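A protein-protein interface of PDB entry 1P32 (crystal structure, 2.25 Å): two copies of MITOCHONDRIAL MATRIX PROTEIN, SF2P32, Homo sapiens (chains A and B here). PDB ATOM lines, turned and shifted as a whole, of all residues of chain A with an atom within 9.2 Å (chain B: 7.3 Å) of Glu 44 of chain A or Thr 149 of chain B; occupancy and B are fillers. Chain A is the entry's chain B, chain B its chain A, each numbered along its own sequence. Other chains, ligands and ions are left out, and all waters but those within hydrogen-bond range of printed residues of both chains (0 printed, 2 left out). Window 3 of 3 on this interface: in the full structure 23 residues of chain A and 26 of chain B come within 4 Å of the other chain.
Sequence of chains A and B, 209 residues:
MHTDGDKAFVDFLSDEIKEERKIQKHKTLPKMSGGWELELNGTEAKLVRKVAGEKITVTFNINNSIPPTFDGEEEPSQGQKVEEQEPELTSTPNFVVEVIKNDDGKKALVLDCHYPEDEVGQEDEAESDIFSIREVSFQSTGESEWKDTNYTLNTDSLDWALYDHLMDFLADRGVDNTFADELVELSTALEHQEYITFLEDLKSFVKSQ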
ATOM      1  N   LEU A  38      11.941  24.722  15.601  1.00  0.00           N
ATOM      2  CA  LEU A  38      12.024  23.436  14.915  1.00  0.00           C
ATOM      3  C   LEU A  38      13.248  22.603  15.299  1.00  0.00           C
ATOM      4  O   LEU A  38      14.356  23.116  15.413  1.00  0.00           O
ATOM      5  CB  LEU A  38      12.028  23.664  13.397  1.00  0.00           C
ATOM      6  CG  LEU A  38      12.161  22.433  12.488  1.00  0.00           C
ATOM      7  CD1 LEU A  38      10.940  21.535  12.667  1.00  0.00           C
ATOM      8  CD2 LEU A  38      12.271  22.878  11.034  1.00  0.00           C
ATOM      9  N   GLU A  39      13.028  21.310  15.497  1.00  0.00           N
ATOM     10  CA  GLU A  39      14.091  20.370  15.826  1.00  0.00           C
ATOM     11  C   GLU A  39      13.928  19.170  14.899  1.00  0.00           C
ATOM     12  O   GLU A  39      12.833  18.626  14.763  1.00  0.00           O
ATOM     13  CB  GLU A  39      13.983  19.927  17.284  1.00  0.00           C
ATOM     14  CG  GLU A  39      14.230  21.050  18.268  1.00  0.00           C
ATOM     15  CD  GLU A  39      14.035  20.618  19.701  1.00  0.00           C
ATOM     16  OE1 GLU A  39      14.659  19.616  20.109  1.00  0.00           O
ATOM     17  OE2 GLU A  39      13.265  21.285  20.420  1.00  0.00           O
ATOM     18  N   LEU A  40      15.018  18.764  14.258  1.00  0.00           N
ATOM     19  CA  LEU A  40      14.974  17.638  13.333  1.00  0.00           C
ATOM     20  C   LEU A  40      15.825  16.455  13.766  1.00  0.00           C
ATOM     21  O   LEU A  40      16.958  16.617  14.206  1.00  0.00           O
ATOM     22  CB  LEU A  40      15.434  18.080  11.944  1.00  0.00           C
ATOM     23  CG  LEU A  40      14.659  19.178  11.216  1.00  0.00           C
ATOM     24  CD1 LEU A  40      15.332  19.447   9.875  1.00  0.00           C
ATOM     25  CD2 LEU A  40      13.209  18.751  11.010  1.00  0.00           C
ATOM     26  N   ASN A  41      15.264  15.261  13.626  1.00  0.00           N
ATOM     27  CA  ASN A  41      15.956  14.026  13.962  1.00  0.00           C
ATOM     28  C   ASN A  41      15.603  13.073  12.830  1.00  0.00           C
ATOM     29  O   ASN A  41      14.630  12.329  12.920  1.00  0.00           O
ATOM     30  CB  ASN A  41      15.446  13.460  15.289  1.00  0.00           C
ATOM     31  CG  ASN A  41      16.128  12.154  15.668  1.00  0.00           C
ATOM     32  OD1 ASN A  41      15.737  11.492  16.632  1.00  0.00           O
ATOM     33  ND2 ASN A  41      17.157  11.781  14.916  1.00  0.00           N
ATOM     34  N   GLY A  42      16.384  13.108  11.757  1.00  0.00           N
ATOM     35  CA  GLY A  42      16.095  12.252  10.620  1.00  0.00           C
ATOM     36  C   GLY A  42      14.834  12.739   9.928  1.00  0.00           C
ATOM     37  O   GLY A  42      14.784  13.869   9.443  1.00  0.00           O
ATOM     38  N   THR A  43      13.811  11.890   9.885  1.00  0.00           N
ATOM     39  CA  THR A  43      12.546  12.243   9.257  1.00  0.00           C
ATOM     40  C   THR A  43      11.555  12.722  10.314  1.00  0.00           C
ATOM     41  O   THR A  43      10.437  13.121   9.996  1.00  0.00           O
ATOM     42  CB  THR A  43      11.931  11.039   8.528  1.00  0.00           C
ATOM     43  OG1 THR A  43      11.817   9.939   9.443  1.00  0.00           O
ATOM     44  CG2 THR A  43      12.791  10.642   7.330  1.00  0.00           C
ATOM     45  N   GLU A  44      11.971  12.670  11.573  1.00  0.00           N
ATOM     46  CA  GLU A  44      11.114  13.104  12.661  1.00  0.00           C
ATOM     47  C   GLU A  44      11.369  14.569  12.987  1.00  0.00           C
ATOM     48  O   GLU A  44      12.503  14.965  13.284  1.00  0.00           O
ATOM     49  CB  GLU A  44      11.363  12.269  13.915  1.00  0.00           C
ATOM     50  CG  GLU A  44      10.431  12.619  15.064  1.00  0.00           C
ATOM     51  CD  GLU A  44      10.802  11.920  16.358  1.00  0.00           C
ATOM     52  OE1 GLU A  44      11.871  12.241  16.923  1.00  0.00           O
ATOM     53  OE2 GLU A  44      10.029  11.046  16.804  1.00  0.00           O
ATOM     54  N   ALA A  45      10.305  15.362  12.930  1.00  0.00           N
ATOM     55  CA  ALA A  45      10.383  16.785  13.227  1.00  0.00           C
ATOM     56  C   ALA A  45       9.576  17.087  14.478  1.00  0.00           C
ATOM     57  O   ALA A  45       8.578  16.432  14.762  1.00  0.00           O
ATOM     58  CB  ALA A  45       9.849  17.597  12.063  1.00  0.00           C
ATOM     59  N   LYS A  46      10.016  18.092  15.220  1.00  0.00           N
ATOM     60  CA  LYS A  46       9.341  18.483  16.437  1.00  0.00           C
ATOM     61  C   LYS A  46       9.261  20.009  16.515  1.00  0.00           C
ATOM     62  O   LYS A  46      10.258  20.701  16.320  1.00  0.00           O
ATOM     63  CB  LYS A  46      10.100  17.915  17.639  1.00  0.00           C
ATOM     64  CG  LYS A  46       9.441  18.156  18.975  1.00  0.00           C
ATOM     65  CD  LYS A  46      10.200  17.476  20.118  1.00  0.00           C
ATOM     66  CE  LYS A  46      10.192  15.948  20.009  1.00  0.00           C
ATOM     67  NZ  LYS A  46      10.918  15.428  18.816  1.00  0.00           N
ATOM     68  N   LEU A  47       8.063  20.522  16.774  1.00  0.00           N
ATOM     69  CA  LEU A  47       7.839  21.957  16.902  1.00  0.00           C
ATOM     70  C   LEU A  47       7.555  22.219  18.369  1.00  0.00           C
ATOM     71  O   LEU A  47       6.618  21.652  18.930  1.00  0.00           O
ATOM     72  CB  LEU A  47       6.637  22.393  16.055  1.00  0.00           C
ATOM     73  CG  LEU A  47       6.791  22.273  14.537  1.00  0.00           C
ATOM     74  CD1 LEU A  47       5.458  22.506  13.852  1.00  0.00           C
ATOM     75  CD2 LEU A  47       7.829  23.281  14.063  1.00  0.00           C
ATOM     76  N   THR A  57       4.318  20.832  22.439  1.00  0.00           N
ATOM     77  CA  THR A  57       5.166  20.139  21.465  1.00  0.00           C
ATOM     78  C   THR A  57       4.359  19.430  20.365  1.00  0.00           C
ATOM     79  O   THR A  57       3.391  18.726  20.642  1.00  0.00           O
ATOM     80  CB  THR A  57       6.069  19.084  22.171  1.00  0.00           C
ATOM     81  OG1 THR A  57       6.880  19.728  23.162  1.00  0.00           O
ATOM     82  CG2 THR A  57       6.983  18.403  21.172  1.00  0.00           C
ATOM     83  N   VAL A  58       4.757  19.619  19.114  1.00  0.00           N
ATOM     84  CA  VAL A  58       4.075  18.958  18.009  1.00  0.00           C
ATOM     85  C   VAL A  58       5.090  18.114  17.245  1.00  0.00           C
ATOM     86  O   VAL A  58       6.082  18.627  16.722  1.00  0.00           O
ATOM     87  CB  VAL A  58       3.422  19.963  17.042  1.00  0.00           C
ATOM     88  CG1 VAL A  58       2.744  19.210  15.912  1.00  0.00           C
ATOM     89  CG2 VAL A  58       2.408  20.824  17.780  1.00  0.00           C
ATOM     90  N   THR A  59       4.829  16.816  17.182  1.00  0.00           N
ATOM     91  CA  THR A  59       5.731  15.891  16.516  1.00  0.00           C
ATOM     92  C   THR A  59       5.116  15.267  15.277  1.00  0.00           C
ATOM     93  O   THR A  59       3.929  14.928  15.267  1.00  0.00           O
ATOM     94  CB  THR A  59       6.137  14.764  17.483  1.00  0.00           C
ATOM     95  OG1 THR A  59       6.788  15.335  18.620  1.00  0.00           O
ATOM     96  CG2 THR A  59       7.087  13.782  16.807  1.00  0.00           C
ATOM     97  N   PHE A  60       5.925  15.122  14.232  1.00  0.00           N
ATOM     98  CA  PHE A  60       5.457  14.504  12.998  1.00  0.00           C
ATOM     99  C   PHE A  60       6.611  13.874  12.223  1.00  0.00           C
ATOM    100  O   PHE A  60       7.752  14.319  12.323  1.00  0.00           O
ATOM    101  CB  PHE A  60       4.708  15.532  12.141  1.00  0.00           C
ATOM    102  CG  PHE A  60       5.568  16.659  11.621  1.00  0.00           C
ATOM    103  CD1 PHE A  60       6.323  16.501  10.465  1.00  0.00           C
ATOM    104  CD2 PHE A  60       5.587  17.892  12.269  1.00  0.00           C
ATOM    105  CE1 PHE A  60       7.076  17.556   9.956  1.00  0.00           C
ATOM    106  CE2 PHE A  60       6.338  18.951  11.769  1.00  0.00           C
ATOM    107  CZ  PHE A  60       7.082  18.786  10.609  1.00  0.00           C
ATOM    108  N   ASN A  61       6.309  12.823  11.465  1.00  0.00           N
ATOM    109  CA  ASN A  61       7.319  12.124  10.680  1.00  0.00           C
ATOM    110  C   ASN A  61       6.907  12.227   9.220  1.00  0.00           C
ATOM    111  O   ASN A  61       5.752  11.965   8.885  1.00  0.00           O
ATOM    112  CB  ASN A  61       7.385  10.651  11.097  1.00  0.00           C
ATOM    113  CG  ASN A  61       8.609   9.939  10.546  1.00  0.00           C
ATOM    114  OD1 ASN A  61       8.881   9.973   9.346  1.00  0.00           O
ATOM    115  ND2 ASN A  61       9.351   9.279  11.426  1.00  0.00           N
ATOM    116  N   ILE A  62       7.839  12.601   8.346  1.00  0.00           N
ATOM    117  CA  ILE A  62       7.503  12.740   6.932  1.00  0.00           C
ATOM    118  C   ILE A  62       7.373  11.431   6.148  1.00  0.00           C
ATOM    119  O   ILE A  62       6.937  11.448   4.996  1.00  0.00           O
ATOM    120  CB  ILE A  62       8.518  13.625   6.185  1.00  0.00           C
ATOM    121  CG1 ILE A  62       9.872  12.919   6.123  1.00  0.00           C
ATOM    122  CG2 ILE A  62       8.631  14.979   6.876  1.00  0.00           C
ATOM    123  CD1 ILE A  62      10.891  13.641   5.296  1.00  0.00           C
ATOM    124  N   ASN A  63       7.746  10.302   6.748  1.00  0.00           N
ATOM    125  CA  ASN A  63       7.633   9.033   6.031  1.00  0.00           C
ATOM    126  C   ASN A  63       6.181   8.646   5.773  1.00  0.00           C
ATOM    127  O   ASN A  63       5.368   8.602   6.694  1.00  0.00           O
ATOM    128  CB  ASN A  63       8.325   7.886   6.780  1.00  0.00           C
ATOM    129  CG  ASN A  63       9.840   7.988   6.747  1.00  0.00           C
ATOM    130  OD1 ASN A  63      10.423   8.407   5.747  1.00  0.00           O
ATOM    131  ND2 ASN A  63      10.486   7.564   7.825  1.00  0.00           N
ATOM    132  N   PRO A  93       1.323  14.756   6.916  1.00  0.00           N
ATOM    133  CA  PRO A  93       1.700  13.865   8.017  1.00  0.00           C
ATOM    134  C   PRO A  93       0.835  13.967   9.271  1.00  0.00           C
ATOM    135  O   PRO A  93       0.478  15.063   9.705  1.00  0.00           O
ATOM    136  CB  PRO A  93       3.136  14.289   8.296  1.00  0.00           C
ATOM    137  CG  PRO A  93       3.039  15.781   8.084  1.00  0.00           C
ATOM    138  CD  PRO A  93       2.372  15.771   6.723  1.00  0.00           C
ATOM    139  N   ASN A  94       0.502  12.815   9.847  1.00  0.00           N
ATOM    140  CA  ASN A  94      -0.277  12.788  11.077  1.00  0.00           C
ATOM    141  C   ASN A  94       0.636  13.462  12.090  1.00  0.00           C
ATOM    142  O   ASN A  94       1.856  13.340  11.997  1.00  0.00           O
ATOM    143  CB  ASN A  94      -0.553  11.345  11.506  1.00  0.00           C
ATOM    144  CG  ASN A  94      -1.256  10.542  10.430  1.00  0.00           C
ATOM    145  OD1 ASN A  94      -2.355  10.886   9.999  1.00  0.00           O
ATOM    146  ND2 ASN A  94      -0.621   9.462   9.985  1.00  0.00           N
ATOM    147  N   VAL A  96       1.319  14.662  16.386  1.00  0.00           N
ATOM    148  CA  VAL A  96       0.966  14.491  17.783  1.00  0.00           C
ATOM    149  C   VAL A  96       1.249  15.740  18.603  1.00  0.00           C
ATOM    150  O   VAL A  96       2.371  16.251  18.619  1.00  0.00           O
ATOM    151  CB  VAL A  96       1.739  13.299  18.413  1.00  0.00           C
ATOM    152  CG1 VAL A  96       1.329  13.118  19.866  1.00  0.00           C
ATOM    153  CG2 VAL A  96       1.462  12.030  17.628  1.00  0.00           C
ATOM    154  N   LEU A 190      10.195  19.581   3.711  1.00  0.00           N
ATOM    155  CA  LEU A 190      11.175  18.701   4.335  1.00  0.00           C
ATOM    156  C   LEU A 190      11.273  17.427   3.511  1.00  0.00           C
ATOM    157  O   LEU A 190      12.358  16.904   3.285  1.00  0.00           O
ATOM    158  CB  LEU A 190      10.764  18.366   5.773  1.00  0.00           C
ATOM    159  CG  LEU A 190      10.997  19.451   6.826  1.00  0.00           C
ATOM    160  CD1 LEU A 190      10.397  19.031   8.156  1.00  0.00           C
ATOM    161  CD2 LEU A 190      12.493  19.683   6.974  1.00  0.00           C
ATOM    162  N   GLU A 194      14.638  15.790   1.677  1.00  0.00           N
ATOM    163  CA  GLU A 194      15.151  14.507   2.120  1.00  0.00           C
ATOM    164  C   GLU A 194      15.110  13.509   0.979  1.00  0.00           C
ATOM    165  O   GLU A 194      15.866  12.543   0.961  1.00  0.00           O
ATOM    166  CB  GLU A 194      14.375  14.009   3.338  1.00  0.00           C
ATOM    167  CG  GLU A 194      14.493  14.981   4.505  1.00  0.00           C
ATOM    168  CD  GLU A 194      14.153  14.365   5.845  1.00  0.00           C
ATOM    169  OE1 GLU A 194      14.086  15.120   6.836  1.00  0.00           O
ATOM    170  OE2 GLU A 194      13.968  13.132   5.914  1.00  0.00           O
ATOM    171  N   GLN B 139      18.997   1.206   5.792  1.00  0.00           N
ATOM    172  CA  GLN B 139      18.889   0.830   7.194  1.00  0.00           C
ATOM    173  C   GLN B 139      20.252   0.320   7.622  1.00  0.00           C
ATOM    174  O   GLN B 139      21.063  -0.061   6.780  1.00  0.00           O
ATOM    175  CB  GLN B 139      17.863  -0.292   7.383  1.00  0.00           C
ATOM    176  CG  GLN B 139      16.417   0.051   7.031  1.00  0.00           C
ATOM    177  CD  GLN B 139      15.800   1.073   7.972  1.00  0.00           C
ATOM    178  OE1 GLN B 139      15.889   0.941   9.191  1.00  0.00           O
ATOM    179  NE2 GLN B 139      15.146   2.084   7.407  1.00  0.00           N
ATOM    180  N   GLU B 143      20.229  -4.126  12.724  1.00  0.00           N
ATOM    181  CA  GLU B 143      19.784  -3.109  13.669  1.00  0.00           C
ATOM    182  C   GLU B 143      18.700  -3.654  14.585  1.00  0.00           C
ATOM    183  O   GLU B 143      18.048  -4.648  14.268  1.00  0.00           O
ATOM    184  CB  GLU B 143      19.244  -1.887  12.923  1.00  0.00           C
ATOM    185  CG  GLU B 143      18.719  -0.793  13.838  1.00  0.00           C
ATOM    186  CD  GLU B 143      18.218   0.415  13.078  1.00  0.00           C
ATOM    187  OE1 GLU B 143      17.313   0.254  12.233  1.00  0.00           O
ATOM    188  OE2 GLU B 143      18.728   1.529  13.328  1.00  0.00           O
ATOM    189  N   TRP B 146      13.491  -1.750  12.505  1.00  0.00           N
ATOM    190  CA  TRP B 146      13.280  -0.733  11.478  1.00  0.00           C
ATOM    191  C   TRP B 146      13.365   0.665  12.094  1.00  0.00           C
ATOM    192  O   TRP B 146      12.513   1.056  12.892  1.00  0.00           O
ATOM    193  CB  TRP B 146      11.909  -0.939  10.821  1.00  0.00           C
ATOM    194  CG  TRP B 146      11.685  -0.124   9.576  1.00  0.00           C
ATOM    195  CD1 TRP B 146      11.749   1.233   9.458  1.00  0.00           C
ATOM    196  CD2 TRP B 146      11.343  -0.625   8.273  1.00  0.00           C
ATOM    197  NE1 TRP B 146      11.470   1.612   8.166  1.00  0.00           N
ATOM    198  CE2 TRP B 146      11.216   0.492   7.417  1.00  0.00           C
ATOM    199  CE3 TRP B 146      11.132  -1.907   7.746  1.00  0.00           C
ATOM    200  CZ2 TRP B 146      10.888   0.367   6.061  1.00  0.00           C
ATOM    201  CZ3 TRP B 146      10.804  -2.032   6.396  1.00  0.00           C
ATOM    202  CH2 TRP B 146      10.686  -0.899   5.571  1.00  0.00           C
ATOM    203  N   LYS B 147      14.407   1.404  11.722  1.00  0.00           N
ATOM    204  CA  LYS B 147      14.630   2.754  12.231  1.00  0.00           C
ATOM    205  C   LYS B 147      13.631   3.699  11.565  1.00  0.00           C
ATOM    206  O   LYS B 147      13.698   3.950  10.359  1.00  0.00           O
ATOM    207  CB  LYS B 147      16.071   3.176  11.932  1.00  0.00           C
ATOM    208  CG  LYS B 147      16.557   4.415  12.664  1.00  0.00           C
ATOM    209  CD  LYS B 147      18.051   4.608  12.425  1.00  0.00           C
ATOM    210  CE  LYS B 147      18.629   5.757  13.241  1.00  0.00           C
ATOM    211  NZ  LYS B 147      18.039   7.071  12.876  1.00  0.00           N
ATOM    212  N   ASP B 148      12.707   4.218  12.368  1.00  0.00           N
ATOM    213  CA  ASP B 148      11.653   5.110  11.892  1.00  0.00           C
ATOM    214  C   ASP B 148      12.106   6.488  11.428  1.00  0.00           C
ATOM    215  O   ASP B 148      11.405   7.143  10.657  1.00  0.00           O
ATOM    216  CB  ASP B 148      10.591   5.270  12.981  1.00  0.00           C
ATOM    217  CG  ASP B 148       9.990   3.944  13.405  1.00  0.00           C
ATOM    218  OD1 ASP B 148       9.396   3.258  12.548  1.00  0.00           O
ATOM    219  OD2 ASP B 148      10.117   3.585  14.595  1.00  0.00           O
ATOM    220  N   THR B 149      13.262   6.941  11.894  1.00  0.00           N
ATOM    221  CA  THR B 149      13.745   8.255  11.489  1.00  0.00           C
ATOM    222  C   THR B 149      14.558   8.225  10.195  1.00  0.00           C
ATOM    223  O   THR B 149      15.063   9.254   9.752  1.00  0.00           O
ATOM    224  CB  THR B 149      14.576   8.917  12.606  1.00  0.00           C
ATOM    225  OG1 THR B 149      15.658   8.056  12.979  1.00  0.00           O
ATOM    226  CG2 THR B 149      13.703   9.184  13.822  1.00  0.00           C
ATOM    227  N   ASN B 150      14.688   7.044   9.592  1.00  0.00           N
ATOM    228  CA  ASN B 150      15.414   6.910   8.330  1.00  0.00           C
ATOM    229  C   ASN B 150      14.452   7.170   7.176  1.00  0.00           C
ATOM    230  O   ASN B 150      13.322   6.678   7.181  1.00  0.00           O
ATOM    231  CB  ASN B 150      16.009   5.505   8.190  1.00  0.00           C
ATOM    232  CG  ASN B 150      17.243   5.302   9.049  1.00  0.00           C
ATOM    233  OD1 ASN B 150      17.773   4.196   9.138  1.00  0.00           O
ATOM    234  ND2 ASN B 150      17.717   6.373   9.672  1.00  0.00           N
ATOM    235  N   TYR B 151      14.900   7.937   6.189  1.00  0.00           N
ATOM    236  CA  TYR B 151      14.058   8.254   5.047  1.00  0.00           C
ATOM    237  C   TYR B 151      13.568   6.993   4.342  1.00  0.00           C
ATOM    238  O   TYR B 151      14.354   6.105   4.015  1.00  0.00           O
ATOM    239  CB  TYR B 151      14.807   9.120   4.034  1.00  0.00           C
ATOM    240  CG  TYR B 151      13.929   9.561   2.878  1.00  0.00           C
ATOM    241  CD1 TYR B 151      12.986  10.585   3.036  1.00  0.00           C
ATOM    242  CD2 TYR B 151      13.992   8.908   1.648  1.00  0.00           C
ATOM    243  CE1 TYR B 151      12.128  10.944   1.992  1.00  0.00           C
ATOM    244  CE2 TYR B 151      13.139   9.257   0.601  1.00  0.00           C
ATOM    245  CZ  TYR B 151      12.212  10.271   0.780  1.00  0.00           C
ATOM    246  OH  TYR B 151      11.369  10.600  -0.255  1.00  0.00           O
ATOM    247  N   THR B 152      12.261   6.935   4.110  1.00  0.00           N
ATOM    248  CA  THR B 152      11.634   5.806   3.434  1.00  0.00           C
ATOM    249  C   THR B 152      10.855   6.329   2.235  1.00  0.00           C
ATOM    250  O   THR B 152       9.928   7.122   2.381  1.00  0.00           O
ATOM    251  CB  THR B 152      10.675   5.061   4.376  1.00  0.00           C
ATOM    252  OG1 THR B 152      11.422   4.521   5.474  1.00  0.00           O
ATOM    253  CG2 THR B 152       9.963   3.930   3.640  1.00  0.00           C
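OG1 of Thr 149 of chain B lies within hydrogen-bond range of NZ of Lys 147 of chain B.
NZ of Lys 147 of chain B sits close to ND2 of Asn 150 of chain B, at 3.3 Å.
The backbone carbonyl oxygen (O) of Asn 150 of chain B sits at hydrogen-bond distance from the side-chain hydroxyl (OG1) of Thr 152 of chain B.
The side-chain hydroxyl (OG1) of Thr 43 of chain A is in hydrogen-bond range of the side-chain amide oxygen (OD1) of Asn 61 of chain A, at 2.9 Å.
The side-chain amide nitrogen of Asn 63 of chain A is in hydrogen-bond range of the side-chain hydroxyl of Thr 43 of chain A.
NZ of Lys 46 of chain A lies within salt-bridge range of OE1 of Glu 44 of chain A, at 3.8 Å.
The side-chain hydroxyl (OG1) of Thr 43 of chain A is in hydrogen-bond range of the backbone carbonyl oxygen (O) of Asp 148 of chain B (3.1 Å).
ND2 of Asn 61 of chain A sits at hydrogen-bond distance from O of Asp 148 of chain B (3.1 Å).
The side-chain amide nitrogen (ND2) of Asn 63 of chain A is in hydrogen-bond range of the backbone carbonyl oxygen (O) of Asp 148 of chain B, at 3.0 Å.
The backbone NH of Thr 43 of chain A is in hydrogen-bond range of the backbone carbonyl oxygen of Thr 149 of chain B, at 2.9 Å.
The backbone carbonyl oxygen of Asn 150 of chain B sits at hydrogen-bond distance from the side-chain amide nitrogen of Asn 63 of chain A (3.0 Å).
OD1 of Asn 63 of chain A lies within hydrogen-bond range of N of Thr 152 of chain B.
No position is printed for both chains.
Of the printed residues of chain B, Asn 41 of chain A touches Thr 149 (3.4 Å).
Printed residues of chain B within 4 Å of Gly 42 of chain A: Thr 149 (3.3 Å).
Of the printed residues of chain B, Thr 43 of chain A touches Asp 148 (3.1 Å), Thr 149 (2.9 Å), Asn 150 (3.9 Å) and Tyr 151 (3.5 Å).
Glu 44 of chain A touches just one residue of chain B: Thr 149 (3.9 Å).
Ile 62 of chain A touches none of the printed residues of chain B.
Pro 93 of chain A touches none of the printed residues of chain B.
Thr 149 of chain B touches just these residues of chain A: Asn 41 (3.4 Å), Gly 42 (3.3 Å), Thr 43 (2.9 Å) and Glu 44 (3.9 Å).
Printed residues of chain A within 4 Å of Thr 152 of chain B: Asn 63.
The nearest residue of chain B that does not touch Glu 44 of chain A is Asp 148 of chain B (5.6 Å).
Among the printed residues, pairs that only touch across the chains: Gly 42 of chain A with Thr 149 of chain B (3.3 Å), Asn 41 of chain A with Thr 149 of chain B (3.4 Å), Thr 43 of chain A with Tyr 151 of chain B (3.5 Å), Asn 63 of chain A with Tyr 151 of chain B (3.7 Å), Glu 194 of chain A with Tyr 151 of chain B (3.7 Å), Thr 43 of chain A with Asn 150 of chain B (3.9 Å) and Glu 44 of chain A with Thr 149 of chain B (3.9 Å).
Of the 22 printed residues of chain A, 7 touch a printed residue of chain B.
Hydrophobic or aromatic side chains of chain B that line the printed part of chain A: Tyr 151.
Along chain B the printed residues that touch a printed residue of chain A span positions 148 to 152.
Among the printed residues, no Asp or Glu carboxylate lies within 4 Å of a Lys or Arg side-chain nitrogen of the other chain.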
